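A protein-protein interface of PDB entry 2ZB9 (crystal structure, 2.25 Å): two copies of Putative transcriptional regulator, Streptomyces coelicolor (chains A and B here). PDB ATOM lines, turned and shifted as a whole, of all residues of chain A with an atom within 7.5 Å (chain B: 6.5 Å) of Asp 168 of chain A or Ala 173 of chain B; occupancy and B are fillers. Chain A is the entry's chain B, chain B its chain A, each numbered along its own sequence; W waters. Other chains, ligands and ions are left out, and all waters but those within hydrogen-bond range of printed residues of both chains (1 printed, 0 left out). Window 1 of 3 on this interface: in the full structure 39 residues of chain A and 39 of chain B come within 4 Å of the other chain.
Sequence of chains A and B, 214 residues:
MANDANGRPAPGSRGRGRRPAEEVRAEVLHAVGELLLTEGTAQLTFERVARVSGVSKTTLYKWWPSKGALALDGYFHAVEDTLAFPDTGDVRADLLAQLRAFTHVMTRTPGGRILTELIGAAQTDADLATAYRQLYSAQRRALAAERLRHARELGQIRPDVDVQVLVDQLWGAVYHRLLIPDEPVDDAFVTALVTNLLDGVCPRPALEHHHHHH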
ATOM      1  N   ARG A 141      14.596   0.750  16.088  1.00  0.00           N
ATOM      2  CA  ARG A 141      14.610   1.472  14.819  1.00  0.00           C
ATOM      3  C   ARG A 141      13.328   1.189  14.030  1.00  0.00           C
ATOM      4  O   ARG A 141      12.749   2.093  13.444  1.00  0.00           O
ATOM      5  CB  ARG A 141      15.825   1.076  13.970  1.00  0.00           C
ATOM      6  CG  ARG A 141      17.179   1.489  14.549  1.00  0.00           C
ATOM      7  CD  ARG A 141      18.300   1.219  13.546  1.00  0.00           C
ATOM      8  NE  ARG A 141      18.180   2.075  12.365  1.00  0.00           N
ATOM      9  CZ  ARG A 141      18.979   3.104  12.095  1.00  0.00           C
ATOM     10  NH1 ARG A 141      19.979   3.411  12.915  1.00  0.00           N
ATOM     11  NH2 ARG A 141      18.766   3.843  11.012  1.00  0.00           N
ATOM     12  N   LEU A 148       7.178   6.957  11.749  1.00  0.00           N
ATOM     13  CA  LEU A 148       7.563   7.922  10.730  1.00  0.00           C
ATOM     14  C   LEU A 148       6.830   7.647   9.416  1.00  0.00           C
ATOM     15  O   LEU A 148       6.385   8.575   8.746  1.00  0.00           O
ATOM     16  CB  LEU A 148       9.084   7.894  10.521  1.00  0.00           C
ATOM     17  CG  LEU A 148       9.928   8.846  11.387  1.00  0.00           C
ATOM     18  CD1 LEU A 148       9.217   9.149  12.684  1.00  0.00           C
ATOM     19  CD2 LEU A 148      11.293   8.229  11.651  1.00  0.00           C
ATOM     20  N   VAL A 163      12.912   7.375   5.909  1.00  0.00           N
ATOM     21  CA  VAL A 163      12.684   7.407   7.354  1.00  0.00           C
ATOM     22  C   VAL A 163      13.809   6.809   8.196  1.00  0.00           C
ATOM     23  O   VAL A 163      13.969   7.167   9.362  1.00  0.00           O
ATOM     24  CB  VAL A 163      11.343   6.711   7.743  1.00  0.00           C
ATOM     25  CG1 VAL A 163      10.169   7.457   7.122  1.00  0.00           C
ATOM     26  CG2 VAL A 163      11.354   5.261   7.300  1.00  0.00           C
ATOM     27  N   GLN A 164      14.585   5.895   7.625  1.00  0.00           N
ATOM     28  CA  GLN A 164      15.684   5.310   8.378  1.00  0.00           C
ATOM     29  C   GLN A 164      16.777   6.354   8.606  1.00  0.00           C
ATOM     30  O   GLN A 164      17.492   6.303   9.609  1.00  0.00           O
ATOM     31  CB  GLN A 164      16.260   4.092   7.655  1.00  0.00           C
ATOM     32  CG  GLN A 164      15.522   2.782   7.935  1.00  0.00           C
ATOM     33  CD  GLN A 164      15.387   2.481   9.421  1.00  0.00           C
ATOM     34  OE1 GLN A 164      16.292   2.749  10.214  1.00  0.00           O
ATOM     35  NE2 GLN A 164      14.254   1.911   9.804  1.00  0.00           N
ATOM     36  N   VAL A 165      16.912   7.303   7.682  1.00  0.00           N
ATOM     37  CA  VAL A 165      17.914   8.353   7.841  1.00  0.00           C
ATOM     38  C   VAL A 165      17.491   9.247   9.006  1.00  0.00           C
ATOM     39  O   VAL A 165      18.322   9.672   9.811  1.00  0.00           O
ATOM     40  CB  VAL A 165      18.054   9.207   6.567  1.00  0.00           C
ATOM     41  CG1 VAL A 165      19.056  10.350   6.802  1.00  0.00           C
ATOM     42  CG2 VAL A 165      18.522   8.331   5.414  1.00  0.00           C
ATOM     43  N   LEU A 166      16.191   9.513   9.100  1.00  0.00           N
ATOM     44  CA  LEU A 166      15.651  10.346  10.172  1.00  0.00           C
ATOM     45  C   LEU A 166      15.925   9.763  11.556  1.00  0.00           C
ATOM     46  O   LEU A 166      16.140  10.499  12.516  1.00  0.00           O
ATOM     47  CB  LEU A 166      14.144  10.521  10.009  1.00  0.00           C
ATOM     48  CG  LEU A 166      13.614  11.205   8.749  1.00  0.00           C
ATOM     49  CD1 LEU A 166      12.101  11.361   8.882  1.00  0.00           C
ATOM     50  CD2 LEU A 166      14.272  12.559   8.566  1.00  0.00           C
ATOM     51  N   VAL A 167      15.904   8.441  11.664  1.00  0.00           N
ATOM     52  CA  VAL A 167      16.164   7.803  12.939  1.00  0.00           C
ATOM     53  C   VAL A 167      17.568   8.162  13.446  1.00  0.00           C
ATOM     54  O   VAL A 167      17.757   8.436  14.632  1.00  0.00           O
ATOM     55  CB  VAL A 167      16.008   6.263  12.823  1.00  0.00           C
ATOM     56  CG1 VAL A 167      16.503   5.586  14.085  1.00  0.00           C
ATOM     57  CG2 VAL A 167      14.535   5.915  12.591  1.00  0.00           C
ATOM     58  N   ASP A 168      18.542   8.179  12.542  1.00  0.00           N
ATOM     59  CA  ASP A 168      19.912   8.513  12.912  1.00  0.00           C
ATOM     60  C   ASP A 168      20.080  10.002  13.229  1.00  0.00           C
ATOM     61  O   ASP A 168      20.913  10.378  14.054  1.00  0.00           O
ATOM     62  CB  ASP A 168      20.872   8.103  11.794  1.00  0.00           C
ATOM     63  CG  ASP A 168      20.885   6.609  11.572  1.00  0.00           C
ATOM     64  OD1 ASP A 168      21.278   5.875  12.507  1.00  0.00           O
ATOM     65  OD2 ASP A 168      20.494   6.161  10.471  1.00  0.00           O
ATOM     66  N   GLN A 169      19.277  10.843  12.587  1.00  0.00           N
ATOM     67  CA  GLN A 169      19.351  12.283  12.808  1.00  0.00           C
ATOM     68  C   GLN A 169      18.540  12.734  14.012  1.00  0.00           C
ATOM     69  O   GLN A 169      18.548  13.908  14.382  1.00  0.00           O
ATOM     70  CB  GLN A 169      18.879  13.024  11.566  1.00  0.00           C
ATOM     71  CG  GLN A 169      19.833  12.891  10.407  1.00  0.00           C
ATOM     72  CD  GLN A 169      19.442  13.765   9.241  1.00  0.00           C
ATOM     73  OE1 GLN A 169      18.452  13.502   8.556  1.00  0.00           O
ATOM     74  NE2 GLN A 169      20.215  14.818   9.011  1.00  0.00           N
ATOM     75  N   LEU A 170      17.836  11.791  14.619  1.00  0.00           N
ATOM     76  CA  LEU A 170      17.024  12.079  15.791  1.00  0.00           C
ATOM     77  C   LEU A 170      17.628  11.306  16.968  1.00  0.00           C
ATOM     78  O   LEU A 170      18.431  11.859  17.731  1.00  0.00           O
ATOM     79  CB  LEU A 170      15.570  11.654  15.534  1.00  0.00           C
ATOM     80  CG  LEU A 170      14.479  12.703  15.259  1.00  0.00           C
ATOM     81  CD1 LEU A 170      15.046  14.008  14.753  1.00  0.00           C
ATOM     82  CD2 LEU A 170      13.490  12.124  14.265  1.00  0.00           C
ATOM     83  N   TRP A 171      17.262  10.031  17.108  1.00  0.00           N
ATOM     84  CA  TRP A 171      17.792   9.209  18.198  1.00  0.00           C
ATOM     85  C   TRP A 171      19.312   9.042  18.070  1.00  0.00           C
ATOM     86  O   TRP A 171      20.022   9.036  19.070  1.00  0.00           O
ATOM     87  CB  TRP A 171      17.098   7.840  18.211  1.00  0.00           C
ATOM     88  CG  TRP A 171      15.628   7.973  18.498  1.00  0.00           C
ATOM     89  CD1 TRP A 171      15.034   8.029  19.728  1.00  0.00           C
ATOM     90  CD2 TRP A 171      14.595   8.241  17.542  1.00  0.00           C
ATOM     91  NE1 TRP A 171      13.700   8.331  19.599  1.00  0.00           N
ATOM     92  CE2 TRP A 171      13.404   8.472  18.265  1.00  0.00           C
ATOM     93  CE3 TRP A 171      14.565   8.326  16.143  1.00  0.00           C
ATOM     94  CZ2 TRP A 171      12.189   8.774  17.639  1.00  0.00           C
ATOM     95  CZ3 TRP A 171      13.355   8.629  15.516  1.00  0.00           C
ATOM     96  CH2 TRP A 171      12.186   8.855  16.270  1.00  0.00           C
ATOM     97  N   GLY A 172      19.804   8.914  16.841  1.00  0.00           N
ATOM     98  CA  GLY A 172      21.236   8.765  16.631  1.00  0.00           C
ATOM     99  C   GLY A 172      22.018   9.938  17.204  1.00  0.00           C
ATOM    100  O   GLY A 172      23.060   9.755  17.824  1.00  0.00           O
ATOM    101  N   ALA A 173      21.505  11.145  16.994  1.00  0.00           N
ATOM    102  CA  ALA A 173      22.142  12.355  17.491  1.00  0.00           C
ATOM    103  C   ALA A 173      22.227  12.329  19.011  1.00  0.00           C
ATOM    104  O   ALA A 173      23.238  12.731  19.583  1.00  0.00           O
ATOM    105  CB  ALA A 173      21.364  13.586  17.032  1.00  0.00           C
ATOM    106  N   VAL A 174      21.166  11.863  19.670  1.00  0.00           N
ATOM    107  CA  VAL A 174      21.176  11.782  21.121  1.00  0.00           C
ATOM    108  C   VAL A 174      22.226  10.759  21.559  1.00  0.00           C
ATOM    109  O   VAL A 174      23.007  11.013  22.476  1.00  0.00           O
ATOM    110  CB  VAL A 174      19.814  11.346  21.695  1.00  0.00           C
ATOM    111  CG1 VAL A 174      19.899  11.305  23.215  1.00  0.00           C
ATOM    112  CG2 VAL A 174      18.712  12.315  21.251  1.00  0.00           C
ATOM    113  N   TYR A 175      22.240   9.600  20.908  1.00  0.00           N
ATOM    114  CA  TYR A 175      23.213   8.570  21.250  1.00  0.00           C
ATOM    115  C   TYR A 175      24.614   9.148  21.144  1.00  0.00           C
ATOM    116  O   TYR A 175      25.464   8.912  22.001  1.00  0.00           O
ATOM    117  CB  TYR A 175      23.096   7.380  20.301  1.00  0.00           C
ATOM    118  CG  TYR A 175      22.058   6.366  20.703  1.00  0.00           C
ATOM    119  CD1 TYR A 175      22.242   5.569  21.829  1.00  0.00           C
ATOM    120  CD2 TYR A 175      20.899   6.187  19.949  1.00  0.00           C
ATOM    121  CE1 TYR A 175      21.302   4.616  22.196  1.00  0.00           C
ATOM    122  CE2 TYR A 175      19.951   5.234  20.306  1.00  0.00           C
ATOM    123  CZ  TYR A 175      20.161   4.452  21.431  1.00  0.00           C
ATOM    124  OH  TYR A 175      19.237   3.500  21.788  1.00  0.00           O
ATOM    125  N   HIS A 176      24.847   9.920  20.088  1.00  0.00           N
ATOM    126  CA  HIS A 176      26.154  10.516  19.868  1.00  0.00           C
ATOM    127  C   HIS A 176      26.616  11.409  21.021  1.00  0.00           C
ATOM    128  O   HIS A 176      27.747  11.281  21.487  1.00  0.00           O
ATOM    129  CB  HIS A 176      26.158  11.306  18.558  1.00  0.00           C
ATOM    130  CG  HIS A 176      27.483  11.909  18.229  1.00  0.00           C
ATOM    131  ND1 HIS A 176      27.702  13.269  18.230  1.00  0.00           N
ATOM    132  CD2 HIS A 176      28.665  11.337  17.897  1.00  0.00           C
ATOM    133  CE1 HIS A 176      28.962  13.510  17.908  1.00  0.00           C
ATOM    134  NE2 HIS A 176      29.567  12.354  17.702  1.00  0.00           N
ATOM    135  N   LEU A 193      16.409  19.274  17.725  1.00  0.00           N
ATOM    136  CA  LEU A 193      16.580  18.102  16.881  1.00  0.00           C
ATOM    137  C   LEU A 193      15.358  17.959  15.958  1.00  0.00           C
ATOM    138  O   LEU A 193      15.488  17.827  14.744  1.00  0.00           O
ATOM    139  CB  LEU A 193      16.709  16.875  17.781  1.00  0.00           C
ATOM    140  CG  LEU A 193      17.945  15.973  17.793  1.00  0.00           C
ATOM    141  CD1 LEU A 193      19.216  16.706  17.378  1.00  0.00           C
ATOM    142  CD2 LEU A 193      18.067  15.399  19.193  1.00  0.00           C
ATOM    143  N   LEU A 197      14.881  19.443  11.810  1.00  0.00           N
ATOM    144  CA  LEU A 197      14.529  18.455  10.807  1.00  0.00           C
ATOM    145  C   LEU A 197      13.183  18.698  10.124  1.00  0.00           C
ATOM    146  O   LEU A 197      13.088  18.638   8.896  1.00  0.00           O
ATOM    147  CB  LEU A 197      14.574  17.070  11.457  1.00  0.00           C
ATOM    148  CG  LEU A 197      15.150  15.889  10.676  1.00  0.00           C
ATOM    149  CD1 LEU A 197      16.389  16.297   9.884  1.00  0.00           C
ATOM    150  CD2 LEU A 197      15.476  14.777  11.661  1.00  0.00           C
ATOM    151  N   VAL B 167      25.766  19.646  14.251  1.00  0.00           N
ATOM    152  CA  VAL B 167      26.909  18.750  14.288  1.00  0.00           C
ATOM    153  C   VAL B 167      26.472  17.317  14.599  1.00  0.00           C
ATOM    154  O   VAL B 167      26.924  16.367  13.961  1.00  0.00           O
ATOM    155  CB  VAL B 167      27.937  19.205  15.349  1.00  0.00           C
ATOM    156  CG1 VAL B 167      29.051  18.174  15.463  1.00  0.00           C
ATOM    157  CG2 VAL B 167      28.509  20.572  14.975  1.00  0.00           C
ATOM    158  N   ASP B 168      25.588  17.158  15.579  1.00  0.00           N
ATOM    159  CA  ASP B 168      25.112  15.831  15.953  1.00  0.00           C
ATOM    160  C   ASP B 168      24.159  15.230  14.934  1.00  0.00           C
ATOM    161  O   ASP B 168      24.010  14.013  14.864  1.00  0.00           O
ATOM    162  CB  ASP B 168      24.428  15.890  17.316  1.00  0.00           C
ATOM    163  CG  ASP B 168      25.397  16.228  18.427  1.00  0.00           C
ATOM    164  OD1 ASP B 168      26.276  15.383  18.723  1.00  0.00           O
ATOM    165  OD2 ASP B 168      25.285  17.339  18.988  1.00  0.00           O
ATOM    166  N   GLN B 169      23.507  16.079  14.147  1.00  0.00           N
ATOM    167  CA  GLN B 169      22.574  15.578  13.146  1.00  0.00           C
ATOM    168  C   GLN B 169      23.239  15.257  11.816  1.00  0.00           C
ATOM    169  O   GLN B 169      22.590  14.769  10.889  1.00  0.00           O
ATOM    170  CB  GLN B 169      21.418  16.563  12.964  1.00  0.00           C
ATOM    171  CG  GLN B 169      20.516  16.609  14.194  1.00  0.00           C
ATOM    172  CD  GLN B 169      19.306  17.493  14.005  1.00  0.00           C
ATOM    173  OE1 GLN B 169      19.421  18.710  13.938  1.00  0.00           O
ATOM    174  NE2 GLN B 169      18.136  16.879  13.913  1.00  0.00           N
ATOM    175  N   LEU B 170      24.536  15.534  11.727  1.00  0.00           N
ATOM    176  CA  LEU B 170      25.304  15.218  10.529  1.00  0.00           C
ATOM    177  C   LEU B 170      26.322  14.144  10.899  1.00  0.00           C
ATOM    178  O   LEU B 170      26.075  12.958  10.724  1.00  0.00           O
ATOM    179  CB  LEU B 170      26.048  16.445   9.989  1.00  0.00           C
ATOM    180  CG  LEU B 170      25.345  17.479   9.108  1.00  0.00           C
ATOM    181  CD1 LEU B 170      24.315  16.795   8.218  1.00  0.00           C
ATOM    182  CD2 LEU B 170      24.695  18.522   9.966  1.00  0.00           C
ATOM    183  N   TRP B 171      27.463  14.571  11.429  1.00  0.00           N
ATOM    184  CA  TRP B 171      28.519  13.646  11.828  1.00  0.00           C
ATOM    185  C   TRP B 171      28.044  12.660  12.902  1.00  0.00           C
ATOM    186  O   TRP B 171      28.347  11.470  12.837  1.00  0.00           O
ATOM    187  CB  TRP B 171      29.734  14.451  12.315  1.00  0.00           C
ATOM    188  CG  TRP B 171      30.276  15.317  11.219  1.00  0.00           C
ATOM    189  CD1 TRP B 171      31.109  14.927  10.207  1.00  0.00           C
ATOM    190  CD2 TRP B 171      29.884  16.668  10.919  1.00  0.00           C
ATOM    191  NE1 TRP B 171      31.248  15.940   9.292  1.00  0.00           N
ATOM    192  CE2 TRP B 171      30.508  17.016   9.697  1.00  0.00           C
ATOM    193  CE3 TRP B 171      29.062  17.606  11.556  1.00  0.00           C
ATOM    194  CZ2 TRP B 171      30.330  18.274   9.097  1.00  0.00           C
ATOM    195  CZ3 TRP B 171      28.887  18.857  10.960  1.00  0.00           C
ATOM    196  CH2 TRP B 171      29.521  19.176   9.739  1.00  0.00           C
ATOM    197  N   GLY B 172      27.293  13.154  13.881  1.00  0.00           N
ATOM    198  CA  GLY B 172      26.798  12.276  14.929  1.00  0.00           C
ATOM    199  C   GLY B 172      25.964  11.137  14.364  1.00  0.00           C
ATOM    200  O   GLY B 172      26.052  10.003  14.836  1.00  0.00           O
ATOM    201  N   ALA B 173      25.147  11.449  13.358  1.00  0.00           N
ATOM    202  CA  ALA B 173      24.291  10.460  12.693  1.00  0.00           C
ATOM    203  C   ALA B 173      25.146   9.389  12.025  1.00  0.00           C
ATOM    204  O   ALA B 173      24.787   8.213  12.021  1.00  0.00           O
ATOM    205  CB  ALA B 173      23.407  11.143  11.643  1.00  0.00           C
ATOM    206  N   VAL B 174      26.264   9.807  11.436  1.00  0.00           N
ATOM    207  CA  VAL B 174      27.180   8.877  10.774  1.00  0.00           C
ATOM    208  C   VAL B 174      27.849   7.990  11.827  1.00  0.00           C
ATOM    209  O   VAL B 174      27.896   6.766  11.682  1.00  0.00           O
ATOM    210  CB  VAL B 174      28.294   9.627   9.999  1.00  0.00           C
ATOM    211  CG1 VAL B 174      29.235   8.618   9.327  1.00  0.00           C
ATOM    212  CG2 VAL B 174      27.677  10.558   8.964  1.00  0.00           C
ATOM    213  N   TYR B 175      28.374   8.613  12.881  1.00  0.00           N
ATOM    214  CA  TYR B 175      29.016   7.863  13.952  1.00  0.00           C
ATOM    215  C   TYR B 175      28.045   6.819  14.489  1.00  0.00           C
ATOM    216  O   TYR B 175      28.419   5.672  14.737  1.00  0.00           O
ATOM    217  CB  TYR B 175      29.420   8.791  15.102  1.00  0.00           C
ATOM    218  CG  TYR B 175      30.739   9.517  14.920  1.00  0.00           C
ATOM    219  CD1 TYR B 175      31.940   8.816  14.870  1.00  0.00           C
ATOM    220  CD2 TYR B 175      30.784  10.908  14.817  1.00  0.00           C
ATOM    221  CE1 TYR B 175      33.161   9.481  14.721  1.00  0.00           C
ATOM    222  CE2 TYR B 175      31.997  11.586  14.667  1.00  0.00           C
ATOM    223  CZ  TYR B 175      33.181  10.863  14.618  1.00  0.00           C
ATOM    224  OH  TYR B 175      34.383  11.519  14.455  1.00  0.00           O
ATOM    225  N   HIS B 176      26.789   7.216  14.664  1.00  0.00           N
ATOM    226  CA  HIS B 176      25.797   6.296  15.198  1.00  0.00           C
ATOM    227  C   HIS B 176      25.564   5.091  14.303  1.00  0.00           C
ATOM    228  O   HIS B 176      25.524   3.952  14.778  1.00  0.00           O
ATOM    229  CB  HIS B 176      24.476   7.021  15.444  1.00  0.00           C
ATOM    230  CG  HIS B 176      23.387   6.131  15.948  1.00  0.00           C
ATOM    231  ND1 HIS B 176      22.335   5.720  15.160  1.00  0.00           N
ATOM    232  CD2 HIS B 176      23.194   5.560  17.163  1.00  0.00           C
ATOM    233  CE1 HIS B 176      21.540   4.936  15.867  1.00  0.00           C
ATOM    234  NE2 HIS B 176      22.038   4.824  17.085  1.00  0.00           N
ATOM    235  N   ARG B 177      25.412   5.325  13.008  1.00  0.00           N
ATOM    236  CA  ARG B 177      25.189   4.208  12.106  1.00  0.00           C
ATOM    237  C   ARG B 177      26.466   3.365  12.041  1.00  0.00           C
ATOM    238  O   ARG B 177      26.405   2.157  11.811  1.00  0.00           O
ATOM    239  CB  ARG B 177      24.769   4.707  10.717  1.00  0.00           C
ATOM    240  CG  ARG B 177      24.164   3.622   9.848  1.00  0.00           C
ATOM    241  CD  ARG B 177      23.549   4.158   8.547  1.00  0.00           C
ATOM    242  NE  ARG B 177      22.194   4.692   8.710  1.00  0.00           N
ATOM    243  CZ  ARG B 177      21.340   4.863   7.701  1.00  0.00           C
ATOM    244  NH1 ARG B 177      21.703   4.536   6.468  1.00  0.00           N
ATOM    245  NH2 ARG B 177      20.127   5.359   7.915  1.00  0.00           N
ATOM    246  N   LEU B 178      27.617   3.997  12.272  1.00  0.00           N
ATOM    247  CA  LEU B 178      28.889   3.273  12.262  1.00  0.00           C
ATOM    248  C   LEU B 178      29.080   2.442  13.528  1.00  0.00           C
ATOM    249  O   LEU B 178      29.529   1.301  13.449  1.00  0.00           O
ATOM    250  CB  LEU B 178      30.076   4.231  12.130  1.00  0.00           C
ATOM    251  CG  LEU B 178      30.393   4.814  10.757  1.00  0.00           C
ATOM    252  CD1 LEU B 178      31.446   5.909  10.905  1.00  0.00           C
ATOM    253  CD2 LEU B 178      30.883   3.712   9.830  1.00  0.00           C
ATOM    254  N   ILE B 180      26.773   1.237  15.492  1.00  0.00           N
ATOM    255  CA  ILE B 180      25.803   0.150  15.487  1.00  0.00           C
ATOM    256  C   ILE B 180      25.173   0.123  14.090  1.00  0.00           C
ATOM    257  O   ILE B 180      24.182   0.799  13.800  1.00  0.00           O
ATOM    258  CB  ILE B 180      24.770   0.323  16.640  1.00  0.00           C
ATOM    259  CG1 ILE B 180      23.390  -0.133  16.198  1.00  0.00           C
ATOM    260  CG2 ILE B 180      24.805   1.742  17.175  1.00  0.00           C
ATOM    261  CD1 ILE B 180      22.348   0.121  17.235  1.00  0.00           C
ATOM    262  N   GLU B 183      22.007  -0.193   9.628  1.00  0.00           N
ATOM    263  CA  GLU B 183      21.838   0.329   8.278  1.00  0.00           C
ATOM    264  C   GLU B 183      23.196   0.700   7.690  1.00  0.00           C
ATOM    265  O   GLU B 183      24.129   1.038   8.419  1.00  0.00           O
ATOM    266  CB  GLU B 183      20.932   1.560   8.301  1.00  0.00           C
ATOM    267  CG  GLU B 183      19.515   1.304   8.795  1.00  0.00           C
ATOM    268  CD  GLU B 183      18.747   0.349   7.896  1.00  0.00           C
ATOM    269  OE1 GLU B 183      18.845   0.486   6.662  1.00  0.00           O
ATOM    270  OE2 GLU B 183      18.039  -0.531   8.420  1.00  0.00           O
ATOM    271  N   VAL B 185      26.228   2.753   5.617  1.00  0.00           N
ATOM    272  CA  VAL B 185      26.733   4.113   5.545  1.00  0.00           C
ATOM    273  C   VAL B 185      27.281   4.337   4.137  1.00  0.00           C
ATOM    274  O   VAL B 185      28.436   4.025   3.852  1.00  0.00           O
ATOM    275  CB  VAL B 185      27.872   4.352   6.554  1.00  0.00           C
ATOM    276  CG1 VAL B 185      28.431   5.757   6.380  1.00  0.00           C
ATOM    277  CG2 VAL B 185      27.361   4.157   7.967  1.00  0.00           C
ATOM    278  N   PHE B 189      23.119   7.870   1.979  1.00  0.00           N
ATOM    279  CA  PHE B 189      22.912   8.209   3.374  1.00  0.00           C
ATOM    280  C   PHE B 189      23.460   9.615   3.619  1.00  0.00           C
ATOM    281  O   PHE B 189      22.766  10.489   4.140  1.00  0.00           O
ATOM    282  CB  PHE B 189      23.627   7.184   4.257  1.00  0.00           C
ATOM    283  CG  PHE B 189      23.684   7.558   5.707  1.00  0.00           C
ATOM    284  CD1 PHE B 189      22.524   7.833   6.417  1.00  0.00           C
ATOM    285  CD2 PHE B 189      24.906   7.610   6.371  1.00  0.00           C
ATOM    286  CE1 PHE B 189      22.578   8.155   7.772  1.00  0.00           C
ATOM    287  CE2 PHE B 189      24.973   7.930   7.726  1.00  0.00           C
ATOM    288  CZ  PHE B 189      23.803   8.202   8.427  1.00  0.00           C
ATOM    289  N   LEU B 193      21.381  13.107   4.622  1.00  0.00           N
ATOM    290  CA  LEU B 193      21.606  13.803   5.886  1.00  0.00           C
ATOM    291  C   LEU B 193      21.590  15.310   5.671  1.00  0.00           C
ATOM    292  O   LEU B 193      20.982  16.046   6.439  1.00  0.00           O
ATOM    293  CB  LEU B 193      22.954  13.412   6.495  1.00  0.00           C
ATOM    294  CG  LEU B 193      23.155  11.990   7.022  1.00  0.00           C
ATOM    295  CD1 LEU B 193      24.600  11.863   7.525  1.00  0.00           C
ATOM    296  CD2 LEU B 193      22.170  11.695   8.151  1.00  0.00           C
HETATM  297  O   HOH W   1      21.080   1.511  14.844  1.00  0.00           O
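The side-chain carboxylate (OD1) of Asp 168 of chain B is in hydrogen-bond range of a ring nitrogen (ND1) of His 176 of chain A (2.6 Å).
O of Gln 169 of chain B sits at hydrogen-bond distance from NE2 of Gln 169 of chain A (3.0 Å).
The backbone carbonyl oxygen (O) of Leu 193 of chain A is in hydrogen-bond range of the side-chain amide nitrogen (NE2) of Gln 169 of chain B (2.9 Å).
The side-chain carboxylate of Asp 168 of chain A is in hydrogen-bond range of a ring nitrogen (ND1) of His 176 of chain B (2.9 Å).
The backbone carbonyl oxygen (O) of Gln 164 of chain A sits at hydrogen-bond distance from the guanidinium group (NH2) of Arg 177 of chain B.
The guanidinium group (NH2) of Arg 177 of chain B is in salt-bridge range of the side-chain carboxylate (OD2) of Asp 168 of chain A, at 2.7 Å.
O of Leu 193 of chain B is in hydrogen-bond range of NE2 of Gln 169 of chain A (3.0 Å).
The backbone carbonyl oxygen of Asp 168 of chain B sits at hydrogen-bond distance from the backbone NH of Ala 173 of chain B, 3.2 Å away.
The guanidinium group of Arg 141 of chain A is in salt-bridge range of the side-chain carboxylate of Asp 168 of chain A (2.8 Å).
O of Val 167 of chain A lies within hydrogen-bond range of N of Gly 172 of chain A (3.0 Å).
NH2 of Arg 141 of chain A touches NH2 of Arg 177 of chain B (3.7 Å).
Arg 141 of chain A touches Glu 183 of chain B (NH2 to CG, 3.5 Å).
CA of Val 165 of chain A touches NH2 of Arg 177 of chain B (3.7 Å).
Phe 189 of chain B touches Asp 168 of chain A.
CA of Gly 172 of chain A touches CG of His 176 of chain B, 3.5 Å away.
CB of Ala 173 of chain A touches O of Asp 168 of chain B, at 3.4 Å.
CD2 of Tyr 175 of chain B touches NE2 of His 176 of chain A, 3.4 Å away.
Ala 173 of chain B touches just one residue of chain A: Asp 168.
Gly 172 of chain B touches just one residue of chain A: His 176.
Printed residues of chain B within 4 Å of Gln 164 of chain A: Arg 177 (3.3 Å) and Glu 183 (3.8 Å).
Of the printed residues of chain B, His 176 of chain A touches Asp 168, Gly 172 and Tyr 175.
Printed residues of chain B within 4 Å of Leu 193 of chain A: Gln 169.
Printed residues of chain A within 4 Å of Phe 189 of chain B: Asp 168.
Val 167 of chain B touches none of the printed residues of chain A.
The nearest residue of chain B that does not touch Asp 168 of chain A is Asp 168 of chain B (4.8 Å).
The nearest printed residue of chain B that does not touch Leu 193 of chain A is Asp 168 of chain B (5.3 Å).
Hydrophobic or aromatic side chains of chain A that line the printed part of chain B: Val 165, Ala 173, Tyr 175, His 176 and Leu 193.
Hydrophobic or aromatic side chains of chain B within 4 Å of the printed part of chain A: Ala 173, Tyr 175, His 176, Phe 189 and Leu 193.
Among the printed residues, Asp or Glu carboxylates within 4 Å of a Lys or Arg side-chain nitrogen of the other chain: Asp 168 of chain A with Arg 177 of chain B.
Gln 169 of chain A touches its own counterpart, Gln 169 of chain B.
Gln 169 of chain A touches Leu 193 of chain B, and with the chains exchanged Leu 193 of chain A touches Gln 169 of chain B.
Gly 172 of chain A touches His 176 of chain B, and with the chains exchanged His 176 of chain A touches Gly 172 of chain B.
Of the 20 pairs that touch across the chains among the printed residues, 11 have their exchanged pair printed and touching as well.
Water W1 lies within hydrogen-bond range of NH1 of Arg 141 of chain A (2.9 Å) and O of Ile 180 of chain B (3.3 Å).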
